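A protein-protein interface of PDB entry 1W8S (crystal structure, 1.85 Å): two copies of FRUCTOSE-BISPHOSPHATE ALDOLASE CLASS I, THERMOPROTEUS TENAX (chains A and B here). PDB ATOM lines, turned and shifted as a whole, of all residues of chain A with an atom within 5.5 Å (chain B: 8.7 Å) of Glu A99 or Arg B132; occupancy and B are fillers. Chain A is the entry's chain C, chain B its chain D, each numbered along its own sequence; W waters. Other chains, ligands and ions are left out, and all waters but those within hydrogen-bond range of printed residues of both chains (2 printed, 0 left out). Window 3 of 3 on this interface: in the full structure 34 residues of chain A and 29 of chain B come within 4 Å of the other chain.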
ATOM      1  N   ARG A  62     -24.004  30.407  27.352  1.00  0.00           N
ATOM      2  CA  ARG A  62     -23.820  29.309  26.422  1.00  0.00           C
ATOM      3  C   ARG A  62     -23.537  27.937  27.058  1.00  0.00           C
ATOM      4  O   ARG A  62     -23.983  26.925  26.554  1.00  0.00           O
ATOM      5  CB  ARG A  62     -22.700  29.617  25.435  1.00  0.00           C
ATOM      6  CG  ARG A  62     -21.292  29.670  26.056  1.00  0.00           C
ATOM      7  CD  ARG A  62     -20.169  29.737  25.027  1.00  0.00           C
ATOM      8  NE  ARG A  62     -20.340  28.701  24.018  1.00  0.00           N
ATOM      9  CZ  ARG A  62     -19.889  28.803  22.765  1.00  0.00           C
ATOM     10  NH1 ARG A  62     -19.216  29.861  22.362  1.00  0.00           N
ATOM     11  NH2 ARG A  62     -20.117  27.832  21.914  1.00  0.00           N
ATOM     12  N   SER A  97     -21.325  33.550  19.769  1.00  0.00           N
ATOM     13  CA  SER A  97     -21.813  34.244  18.567  1.00  0.00           C
ATOM     14  C   SER A  97     -23.304  34.004  18.435  1.00  0.00           C
ATOM     15  O   SER A  97     -23.819  33.021  18.977  1.00  0.00           O
ATOM     16  CB  SER A  97     -21.131  33.703  17.305  1.00  0.00           C
ATOM     17  OG  SER A  97     -21.448  32.347  17.067  1.00  0.00           O
ATOM     18  N   VAL A  98     -23.961  34.830  17.630  1.00  0.00           N
ATOM     19  CA  VAL A  98     -25.366  34.626  17.335  1.00  0.00           C
ATOM     20  C   VAL A  98     -25.577  33.306  16.625  1.00  0.00           C
ATOM     21  O   VAL A  98     -26.539  32.569  16.927  1.00  0.00           O
ATOM     22  CB  VAL A  98     -25.940  35.787  16.534  1.00  0.00           C
ATOM     23  CG1 VAL A  98     -27.348  35.423  15.985  1.00  0.00           C
ATOM     24  CG2 VAL A  98     -25.949  37.062  17.392  1.00  0.00           C
ATOM     25  N   GLU A  99     -24.688  32.971  15.699  1.00  0.00           N
ATOM     26  CA  GLU A  99     -24.762  31.699  14.986  1.00  0.00           C
ATOM     27  C   GLU A  99     -24.755  30.491  15.940  1.00  0.00           C
ATOM     28  O   GLU A  99     -25.591  29.570  15.823  1.00  0.00           O
ATOM     29  CB  GLU A  99     -23.614  31.555  13.986  1.00  0.00           C
ATOM     30  CG  GLU A  99     -23.665  30.267  13.175  1.00  0.00           C
ATOM     31  CD  GLU A  99     -22.719  30.225  11.988  1.00  0.00           C
ATOM     32  OE1 GLU A  99     -22.240  31.294  11.575  1.00  0.00           O
ATOM     33  OE2 GLU A  99     -22.517  29.103  11.458  1.00  0.00           O
ATOM     34  N   GLU A 100     -23.859  30.525  16.915  1.00  0.00           N
ATOM     35  CA  GLU A 100     -23.799  29.442  17.909  1.00  0.00           C
ATOM     36  C   GLU A 100     -25.093  29.421  18.746  1.00  0.00           C
ATOM     37  O   GLU A 100     -25.622  28.353  19.063  1.00  0.00           O
ATOM     38  CB  GLU A 100     -22.580  29.604  18.795  1.00  0.00           C
ATOM     39  CG  GLU A 100     -21.271  29.272  18.078  1.00  0.00           C
ATOM     40  CD  GLU A 100     -20.072  29.726  18.867  1.00  0.00           C
ATOM     41  OE1 GLU A 100     -19.885  30.961  18.901  1.00  0.00           O
ATOM     42  OE2 GLU A 100     -19.318  28.867  19.379  1.00  0.00           O
ATOM     43  N   ALA A 101     -25.596  30.590  19.119  1.00  0.00           N
ATOM     44  CA  ALA A 101     -26.846  30.675  19.903  1.00  0.00           C
ATOM     45  C   ALA A 101     -28.002  30.020  19.149  1.00  0.00           C
ATOM     46  O   ALA A 101     -28.830  29.320  19.721  1.00  0.00           O
ATOM     47  CB  ALA A 101     -27.183  32.102  20.210  1.00  0.00           C
ATOM     48  N   VAL A 102     -28.055  30.233  17.842  1.00  0.00           N
ATOM     49  CA  VAL A 102     -29.077  29.580  17.032  1.00  0.00           C
ATOM     50  C   VAL A 102     -28.921  28.058  17.137  1.00  0.00           C
ATOM     51  O   VAL A 102     -29.909  27.328  17.304  1.00  0.00           O
ATOM     52  CB  VAL A 102     -28.992  30.027  15.554  1.00  0.00           C
ATOM     53  CG1 VAL A 102     -29.888  29.168  14.659  1.00  0.00           C
ATOM     54  CG2 VAL A 102     -29.372  31.436  15.432  1.00  0.00           C
ATOM     55  N   SER A 103     -27.698  27.571  17.002  1.00  0.00           N
ATOM     56  CA  SER A 103     -27.417  26.139  17.107  1.00  0.00           C
ATOM     57  C   SER A 103     -27.748  25.566  18.481  1.00  0.00           C
ATOM     58  O   SER A 103     -28.079  24.370  18.604  1.00  0.00           O
ATOM     59  CB  SER A 103     -25.954  25.864  16.790  1.00  0.00           C
ATOM     60  OG  SER A 103     -25.631  24.515  17.066  1.00  0.00           O
ATOM     61  N   LEU A 104     -27.651  26.395  19.510  1.00  0.00           N
ATOM     62  CA  LEU A 104     -27.999  25.980  20.882  1.00  0.00           C
ATOM     63  C   LEU A 104     -29.495  25.992  21.192  1.00  0.00           C
ATOM     64  O   LEU A 104     -29.876  25.596  22.278  1.00  0.00           O
ATOM     65  CB  LEU A 104     -27.252  26.852  21.875  1.00  0.00           C
ATOM     66  CG  LEU A 104     -25.737  26.652  21.876  1.00  0.00           C
ATOM     67  CD1 LEU A 104     -25.141  27.730  22.715  1.00  0.00           C
ATOM     68  CD2 LEU A 104     -25.359  25.266  22.409  1.00  0.00           C
ATOM     69  N   ASP A 133     -25.729  40.382  13.122  1.00  0.00           N
ATOM     70  CA  ASP A 133     -25.975  38.939  13.094  1.00  0.00           C
ATOM     71  C   ASP A 133     -27.396  38.570  13.532  1.00  0.00           C
ATOM     72  O   ASP A 133     -27.956  37.618  13.029  1.00  0.00           O
ATOM     73  CB  ASP A 133     -25.002  38.194  13.970  1.00  0.00           C
ATOM     74  CG  ASP A 133     -23.656  37.985  13.324  1.00  0.00           C
ATOM     75  OD1 ASP A 133     -23.531  38.184  12.084  1.00  0.00           O
ATOM     76  OD2 ASP A 133     -22.679  37.605  14.008  1.00  0.00           O
ATOM     77  N   PHE A 137     -29.817  36.237  11.280  1.00  0.00           N
ATOM     78  CA  PHE A 137     -30.348  34.956  11.764  1.00  0.00           C
ATOM     79  C   PHE A 137     -31.786  35.041  12.253  1.00  0.00           C
ATOM     80  O   PHE A 137     -32.356  34.029  12.665  1.00  0.00           O
ATOM     81  CB  PHE A 137     -29.446  34.433  12.869  1.00  0.00           C
ATOM     82  CG  PHE A 137     -28.131  33.871  12.338  1.00  0.00           C
ATOM     83  CD1 PHE A 137     -28.088  32.586  11.813  1.00  0.00           C
ATOM     84  CD2 PHE A 137     -26.976  34.653  12.311  1.00  0.00           C
ATOM     85  CE1 PHE A 137     -26.881  32.060  11.343  1.00  0.00           C
ATOM     86  CE2 PHE A 137     -25.772  34.151  11.809  1.00  0.00           C
ATOM     87  CZ  PHE A 137     -25.731  32.856  11.313  1.00  0.00           C
ATOM     88  N   LEU B   4     -19.001  16.411  23.987  1.00  0.00           N
ATOM     89  CA  LEU B   4     -17.549  16.409  24.127  1.00  0.00           C
ATOM     90  C   LEU B   4     -17.108  16.073  25.543  1.00  0.00           C
ATOM     91  O   LEU B   4     -15.986  15.606  25.734  1.00  0.00           O
ATOM     92  CB  LEU B   4     -16.951  17.722  23.632  1.00  0.00           C
ATOM     93  CG  LEU B   4     -16.976  17.850  22.109  1.00  0.00           C
ATOM     94  CD1 LEU B   4     -16.650  19.262  21.711  1.00  0.00           C
ATOM     95  CD2 LEU B   4     -15.987  16.916  21.483  1.00  0.00           C
ATOM     96  N   VAL B  98      -6.702  25.737  17.741  1.00  0.00           N
ATOM     97  CA  VAL B  98      -7.280  24.382  17.800  1.00  0.00           C
ATOM     98  C   VAL B  98      -6.930  23.511  16.582  1.00  0.00           C
ATOM     99  O   VAL B  98      -6.606  22.336  16.736  1.00  0.00           O
ATOM    100  CB  VAL B  98      -8.803  24.469  17.970  1.00  0.00           C
ATOM    101  CG1 VAL B  98      -9.458  23.110  17.819  1.00  0.00           C
ATOM    102  CG2 VAL B  98      -9.114  25.105  19.365  1.00  0.00           C
ATOM    103  N   VAL B 109      -7.982  20.140  24.031  1.00  0.00           N
ATOM    104  CA  VAL B 109      -7.278  21.408  24.196  1.00  0.00           C
ATOM    105  C   VAL B 109      -7.560  21.990  25.556  1.00  0.00           C
ATOM    106  O   VAL B 109      -8.610  21.779  26.115  1.00  0.00           O
ATOM    107  CB  VAL B 109      -7.601  22.412  23.070  1.00  0.00           C
ATOM    108  CG1 VAL B 109      -7.043  21.944  21.766  1.00  0.00           C
ATOM    109  CG2 VAL B 109      -9.110  22.758  22.945  1.00  0.00           C
ATOM    110  N   GLU B 125     -12.863  36.756  25.431  1.00  0.00           N
ATOM    111  CA  GLU B 125     -12.977  37.051  23.997  1.00  0.00           C
ATOM    112  C   GLU B 125     -12.310  35.942  23.200  1.00  0.00           C
ATOM    113  O   GLU B 125     -12.873  35.409  22.209  1.00  0.00           O
ATOM    114  CB  GLU B 125     -12.233  38.359  23.736  1.00  0.00           C
ATOM    115  CG  GLU B 125     -12.520  39.195  22.540  1.00  0.00           C
ATOM    116  CD  GLU B 125     -11.831  40.566  22.733  1.00  0.00           C
ATOM    117  OE1 GLU B 125     -12.497  41.564  23.120  1.00  0.00           O
ATOM    118  OE2 GLU B 125     -10.595  40.612  22.595  1.00  0.00           O
ATOM    119  N   GLU B 126     -11.088  35.605  23.604  1.00  0.00           N
ATOM    120  CA  GLU B 126     -10.348  34.542  22.953  1.00  0.00           C
ATOM    121  C   GLU B 126     -10.959  33.170  23.132  1.00  0.00           C
ATOM    122  O   GLU B 126     -11.089  32.399  22.178  1.00  0.00           O
ATOM    123  CB  GLU B 126      -8.899  34.559  23.395  1.00  0.00           C
ATOM    124  CG  GLU B 126      -8.031  33.678  22.551  1.00  0.00           C
ATOM    125  CD  GLU B 126      -6.585  34.082  22.624  1.00  0.00           C
ATOM    126  OE1 GLU B 126      -6.003  33.950  23.728  1.00  0.00           O
ATOM    127  OE2 GLU B 126      -6.053  34.505  21.570  1.00  0.00           O
ATOM    128  N   LEU B 127     -11.381  32.874  24.353  1.00  0.00           N
ATOM    129  CA  LEU B 127     -11.973  31.598  24.630  1.00  0.00           C
ATOM    130  C   LEU B 127     -13.182  31.385  23.731  1.00  0.00           C
ATOM    131  O   LEU B 127     -13.469  30.266  23.371  1.00  0.00           O
ATOM    132  CB  LEU B 127     -12.408  31.506  26.083  1.00  0.00           C
ATOM    133  CG  LEU B 127     -12.897  30.131  26.556  1.00  0.00           C
ATOM    134  CD1 LEU B 127     -11.884  29.018  26.210  1.00  0.00           C
ATOM    135  CD2 LEU B 127     -13.153  30.127  28.069  1.00  0.00           C
ATOM    136  N   ALA B 128     -13.897  32.449  23.385  1.00  0.00           N
ATOM    137  CA  ALA B 128     -15.086  32.301  22.569  1.00  0.00           C
ATOM    138  C   ALA B 128     -14.712  31.660  21.257  1.00  0.00           C
ATOM    139  O   ALA B 128     -15.434  30.814  20.731  1.00  0.00           O
ATOM    140  CB  ALA B 128     -15.718  33.632  22.285  1.00  0.00           C
ATOM    141  N   ARG B 129     -13.603  32.116  20.708  1.00  0.00           N
ATOM    142  CA  ARG B 129     -13.122  31.619  19.419  1.00  0.00           C
ATOM    143  C   ARG B 129     -12.598  30.182  19.533  1.00  0.00           C
ATOM    144  O   ARG B 129     -12.879  29.306  18.709  1.00  0.00           O
ATOM    145  CB  ARG B 129     -12.028  32.550  18.931  1.00  0.00           C
ATOM    146  CG  ARG B 129     -12.551  33.942  18.523  1.00  0.00           C
ATOM    147  CD  ARG B 129     -11.447  34.816  17.806  1.00  0.00           C
ATOM    148  NE  ARG B 129     -11.038  35.975  18.610  1.00  0.00           N
ATOM    149  CZ  ARG B 129      -9.888  36.083  19.288  1.00  0.00           C
ATOM    150  NH1 ARG B 129      -8.971  35.098  19.271  1.00  0.00           N
ATOM    151  NH2 ARG B 129      -9.650  37.189  19.996  1.00  0.00           N
ATOM    152  N   ILE B 130     -11.860  29.943  20.598  1.00  0.00           N
ATOM    153  CA  ILE B 130     -11.358  28.608  20.892  1.00  0.00           C
ATOM    154  C   ILE B 130     -12.478  27.599  21.108  1.00  0.00           C
ATOM    155  O   ILE B 130     -12.424  26.506  20.561  1.00  0.00           O
ATOM    156  CB  ILE B 130     -10.389  28.651  22.081  1.00  0.00           C
ATOM    157  CG1 ILE B 130      -9.100  29.364  21.635  1.00  0.00           C
ATOM    158  CG2 ILE B 130     -10.074  27.243  22.561  1.00  0.00           C
ATOM    159  CD1 ILE B 130      -8.329  29.807  22.746  1.00  0.00           C
ATOM    160  N   LYS B 131     -13.494  27.966  21.886  1.00  0.00           N
ATOM    161  CA  LYS B 131     -14.630  27.101  22.120  1.00  0.00           C
ATOM    162  C   LYS B 131     -15.297  26.732  20.805  1.00  0.00           C
ATOM    163  O   LYS B 131     -15.642  25.573  20.542  1.00  0.00           O
ATOM    164  CB  LYS B 131     -15.615  27.776  23.113  1.00  0.00           C
ATOM    165  CG  LYS B 131     -16.966  27.161  23.190  1.00  0.00           C
ATOM    166  CD  LYS B 131     -16.952  25.738  23.783  1.00  0.00           C
ATOM    167  CE  LYS B 131     -18.322  25.132  23.872  1.00  0.00           C
ATOM    168  NZ  LYS B 131     -18.287  23.725  24.426  1.00  0.00           N
ATOM    169  N   ARG B 132     -15.528  27.729  19.967  1.00  0.00           N
ATOM    170  CA  ARG B 132     -16.176  27.486  18.677  1.00  0.00           C
ATOM    171  C   ARG B 132     -15.374  26.474  17.838  1.00  0.00           C
ATOM    172  O   ARG B 132     -15.947  25.545  17.223  1.00  0.00           O
ATOM    173  CB  ARG B 132     -16.336  28.812  17.938  1.00  0.00           C
ATOM    174  CG  ARG B 132     -17.245  28.761  16.725  1.00  0.00           C
ATOM    175  CD  ARG B 132     -17.465  30.147  16.189  1.00  0.00           C
ATOM    176  NE  ARG B 132     -18.509  30.226  15.194  1.00  0.00           N
ATOM    177  CZ  ARG B 132     -18.972  31.380  14.694  1.00  0.00           C
ATOM    178  NH1 ARG B 132     -18.480  32.550  15.108  1.00  0.00           N
ATOM    179  NH2 ARG B 132     -19.910  31.355  13.764  1.00  0.00           N
ATOM    180  N   ASP B 133     -14.065  26.672  17.788  1.00  0.00           N
ATOM    181  CA  ASP B 133     -13.169  25.766  17.057  1.00  0.00           C
ATOM    182  C   ASP B 133     -13.165  24.366  17.690  1.00  0.00           C
ATOM    183  O   ASP B 133     -13.141  23.369  16.968  1.00  0.00           O
ATOM    184  CB  ASP B 133     -11.731  26.291  17.011  1.00  0.00           C
ATOM    185  CG  ASP B 133     -11.513  27.358  15.957  1.00  0.00           C
ATOM    186  OD1 ASP B 133     -12.355  27.490  15.045  1.00  0.00           O
ATOM    187  OD2 ASP B 133     -10.497  28.071  15.958  1.00  0.00           O
ATOM    188  N   ALA B 134     -13.179  24.288  19.015  1.00  0.00           N
ATOM    189  CA  ALA B 134     -13.189  22.993  19.692  1.00  0.00           C
ATOM    190  C   ALA B 134     -14.394  22.201  19.216  1.00  0.00           C
ATOM    191  O   ALA B 134     -14.283  21.021  18.883  1.00  0.00           O
ATOM    192  CB  ALA B 134     -13.257  23.156  21.163  1.00  0.00           C
ATOM    193  N   VAL B 135     -15.548  22.857  19.153  1.00  0.00           N
ATOM    194  CA  VAL B 135     -16.752  22.195  18.685  1.00  0.00           C
ATOM    195  C   VAL B 135     -16.573  21.767  17.232  1.00  0.00           C
ATOM    196  O   VAL B 135     -16.889  20.639  16.893  1.00  0.00           O
ATOM    197  CB  VAL B 135     -18.023  23.075  18.887  1.00  0.00           C
ATOM    198  CG1 VAL B 135     -19.267  22.452  18.223  1.00  0.00           C
ATOM    199  CG2 VAL B 135     -18.269  23.299  20.380  1.00  0.00           C
ATOM    200  N   LYS B 136     -16.043  22.658  16.385  1.00  0.00           N
ATOM    201  CA  LYS B 136     -15.886  22.378  14.966  1.00  0.00           C
ATOM    202  C   LYS B 136     -14.960  21.173  14.711  1.00  0.00           C
ATOM    203  O   LYS B 136     -15.208  20.347  13.828  1.00  0.00           O
ATOM    204  CB  LYS B 136     -15.330  23.637  14.300  1.00  0.00           C
ATOM    205  CG  LYS B 136     -14.782  23.467  12.916  1.00  0.00           C
ATOM    206  CD  LYS B 136     -14.394  24.881  12.361  1.00  0.00           C
ATOM    207  CE  LYS B 136     -13.613  24.795  11.045  1.00  0.00           C
ATOM    208  NZ  LYS B 136     -13.108  26.139  10.551  1.00  0.00           N
ATOM    209  N   PHE B 137     -13.864  21.111  15.460  1.00  0.00           N
ATOM    210  CA  PHE B 137     -12.887  20.021  15.323  1.00  0.00           C
ATOM    211  C   PHE B 137     -13.156  18.796  16.232  1.00  0.00           C
ATOM    212  O   PHE B 137     -12.381  17.848  16.217  1.00  0.00           O
ATOM    213  CB  PHE B 137     -11.470  20.541  15.553  1.00  0.00           C
ATOM    214  CG  PHE B 137     -10.946  21.389  14.397  1.00  0.00           C
ATOM    215  CD1 PHE B 137     -10.380  20.783  13.285  1.00  0.00           C
ATOM    216  CD2 PHE B 137     -11.079  22.750  14.397  1.00  0.00           C
ATOM    217  CE1 PHE B 137      -9.896  21.549  12.246  1.00  0.00           C
ATOM    218  CE2 PHE B 137     -10.577  23.543  13.338  1.00  0.00           C
ATOM    219  CZ  PHE B 137     -10.023  22.940  12.269  1.00  0.00           C
ATOM    220  N   ASP B 138     -14.229  18.855  17.003  1.00  0.00           N
ATOM    221  CA  ASP B 138     -14.652  17.803  17.928  1.00  0.00           C
ATOM    222  C   ASP B 138     -13.556  17.404  18.912  1.00  0.00           C
ATOM    223  O   ASP B 138     -13.382  16.209  19.231  1.00  0.00           O
ATOM    224  CB  ASP B 138     -15.195  16.606  17.158  1.00  0.00           C
ATOM    225  CG  ASP B 138     -16.216  15.796  17.944  1.00  0.00           C
ATOM    226  OD1 ASP B 138     -17.187  16.362  18.519  1.00  0.00           O
ATOM    227  OD2 ASP B 138     -16.099  14.557  18.024  1.00  0.00           O
ATOM    228  N   LEU B 139     -12.882  18.417  19.451  1.00  0.00           N
ATOM    229  CA  LEU B 139     -11.886  18.247  20.506  1.00  0.00           C
ATOM    230  C   LEU B 139     -12.474  18.827  21.786  1.00  0.00           C
ATOM    231  O   LEU B 139     -12.830  20.009  21.813  1.00  0.00           O
ATOM    232  CB  LEU B 139     -10.615  19.037  20.142  1.00  0.00           C
ATOM    233  CG  LEU B 139      -9.289  18.317  19.959  1.00  0.00           C
ATOM    234  CD1 LEU B 139      -9.457  17.053  19.197  1.00  0.00           C
ATOM    235  CD2 LEU B 139      -8.281  19.215  19.286  1.00  0.00           C
ATOM    236  N   LEU B 141     -12.789  20.733  25.260  1.00  0.00           N
ATOM    237  CA  LEU B 141     -12.137  21.929  25.798  1.00  0.00           C
ATOM    238  C   LEU B 141     -12.039  21.801  27.309  1.00  0.00           C
ATOM    239  O   LEU B 141     -13.039  21.613  27.975  1.00  0.00           O
ATOM    240  CB  LEU B 141     -12.938  23.177  25.446  1.00  0.00           C
ATOM    241  CG  LEU B 141     -12.550  24.493  26.115  1.00  0.00           C
ATOM    242  CD1 LEU B 141     -11.143  24.896  25.652  1.00  0.00           C
ATOM    243  CD2 LEU B 141     -13.570  25.564  25.791  1.00  0.00           C
ATOM    244  N   LEU B 171     -19.087  29.188  30.538  1.00  0.00           N
ATOM    245  CA  LEU B 171     -18.424  29.603  29.326  1.00  0.00           C
ATOM    246  C   LEU B 171     -18.269  28.455  28.324  1.00  0.00           C
ATOM    247  O   LEU B 171     -17.816  28.707  27.220  1.00  0.00           O
ATOM    248  CB  LEU B 171     -17.041  30.152  29.681  1.00  0.00           C
ATOM    249  CG  LEU B 171     -17.065  31.457  30.469  1.00  0.00           C
ATOM    250  CD1 LEU B 171     -15.641  31.870  30.772  1.00  0.00           C
ATOM    251  CD2 LEU B 171     -17.785  32.564  29.735  1.00  0.00           C
ATOM    252  N   GLY B 172     -18.555  27.220  28.732  1.00  0.00           N
ATOM    253  CA  GLY B 172     -18.650  26.086  27.802  1.00  0.00           C
ATOM    254  C   GLY B 172     -17.595  24.978  27.933  1.00  0.00           C
ATOM    255  O   GLY B 172     -17.431  24.144  27.042  1.00  0.00           O
HETATM  256  O   HOH W   1     -21.541  33.866  12.218  1.00  0.00           O
HETATM  257  O   HOH W   2     -17.793  32.078  19.828  1.00  0.00           O
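The guanidinium group (NH2) of Arg A62 lies within salt-bridge range of the side-chain carboxylate (OE2) of Glu A100 (2.9 Å).
NZ of Lys B131 is in hydrogen-bond range of O of Gly B172 (2.8 Å).
The side-chain hydroxyl (OG) of Ser A97 sits at hydrogen-bond distance from the side-chain carboxylate (OE1) of Glu A100.
3 positions are printed for both chains.
Of the 5 pairs that touch across the chains among the printed residues, none has its exchanged pair printed and touching as well.
Among the printed residues, pairs that only touch across the chains: Glu A100 with Arg B132, Arg A62 with Leu B171, Arg A62 with Lys B131 and Ser A97 with Arg B132.
Of the 21 printed residues of chain B, 3 touch a printed residue of chain A.
Printed residues of chain B that touch a printed residue of chain A: Lys B131, Arg B132 and Leu B171.
Printed residues of chain B within 4 Å of Glu A99: Arg B132.
Arg B132 touches just these residues of chain A: Ser A97 (3.6 Å), Glu A99 (3.2 Å) and Glu A100 (3.3 Å).
Val A98 touches none of the printed residues of chain B.
Of chain B, only Arg B132 (3.3 Å) comes within 4 Å of Glu A100.
Printed residues of chain A within 4 Å of Leu B171: Arg A62 (3.4 Å).
Of the printed residues of chain B, Ser A97 touches Arg B132.
Of the printed residues of chain A, Lys B131 touches Arg A62.
Printed residues of chain B within 4 Å of Arg A62: Lys B131 and Leu B171.
Val B109 touches none of the printed residues of chain A.
The nearest printed residue of chain B that does not touch Glu A99 is Lys B136 (9.2 Å).
The nearest residue of chain A that does not touch Arg B132 is Arg A62 (4.9 Å).
Water W2 lies within hydrogen-bond range of OE1 of Glu A100 and O of Ala B128.
Water W1 lies within hydrogen-bond range of the side-chain carboxylate (OE1) of Glu A99 and the guanidinium group (NH2) of Arg B132.
OE1 of Glu A99 lies within salt-bridge range of NH2 of Arg B132, at 3.2 Å.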
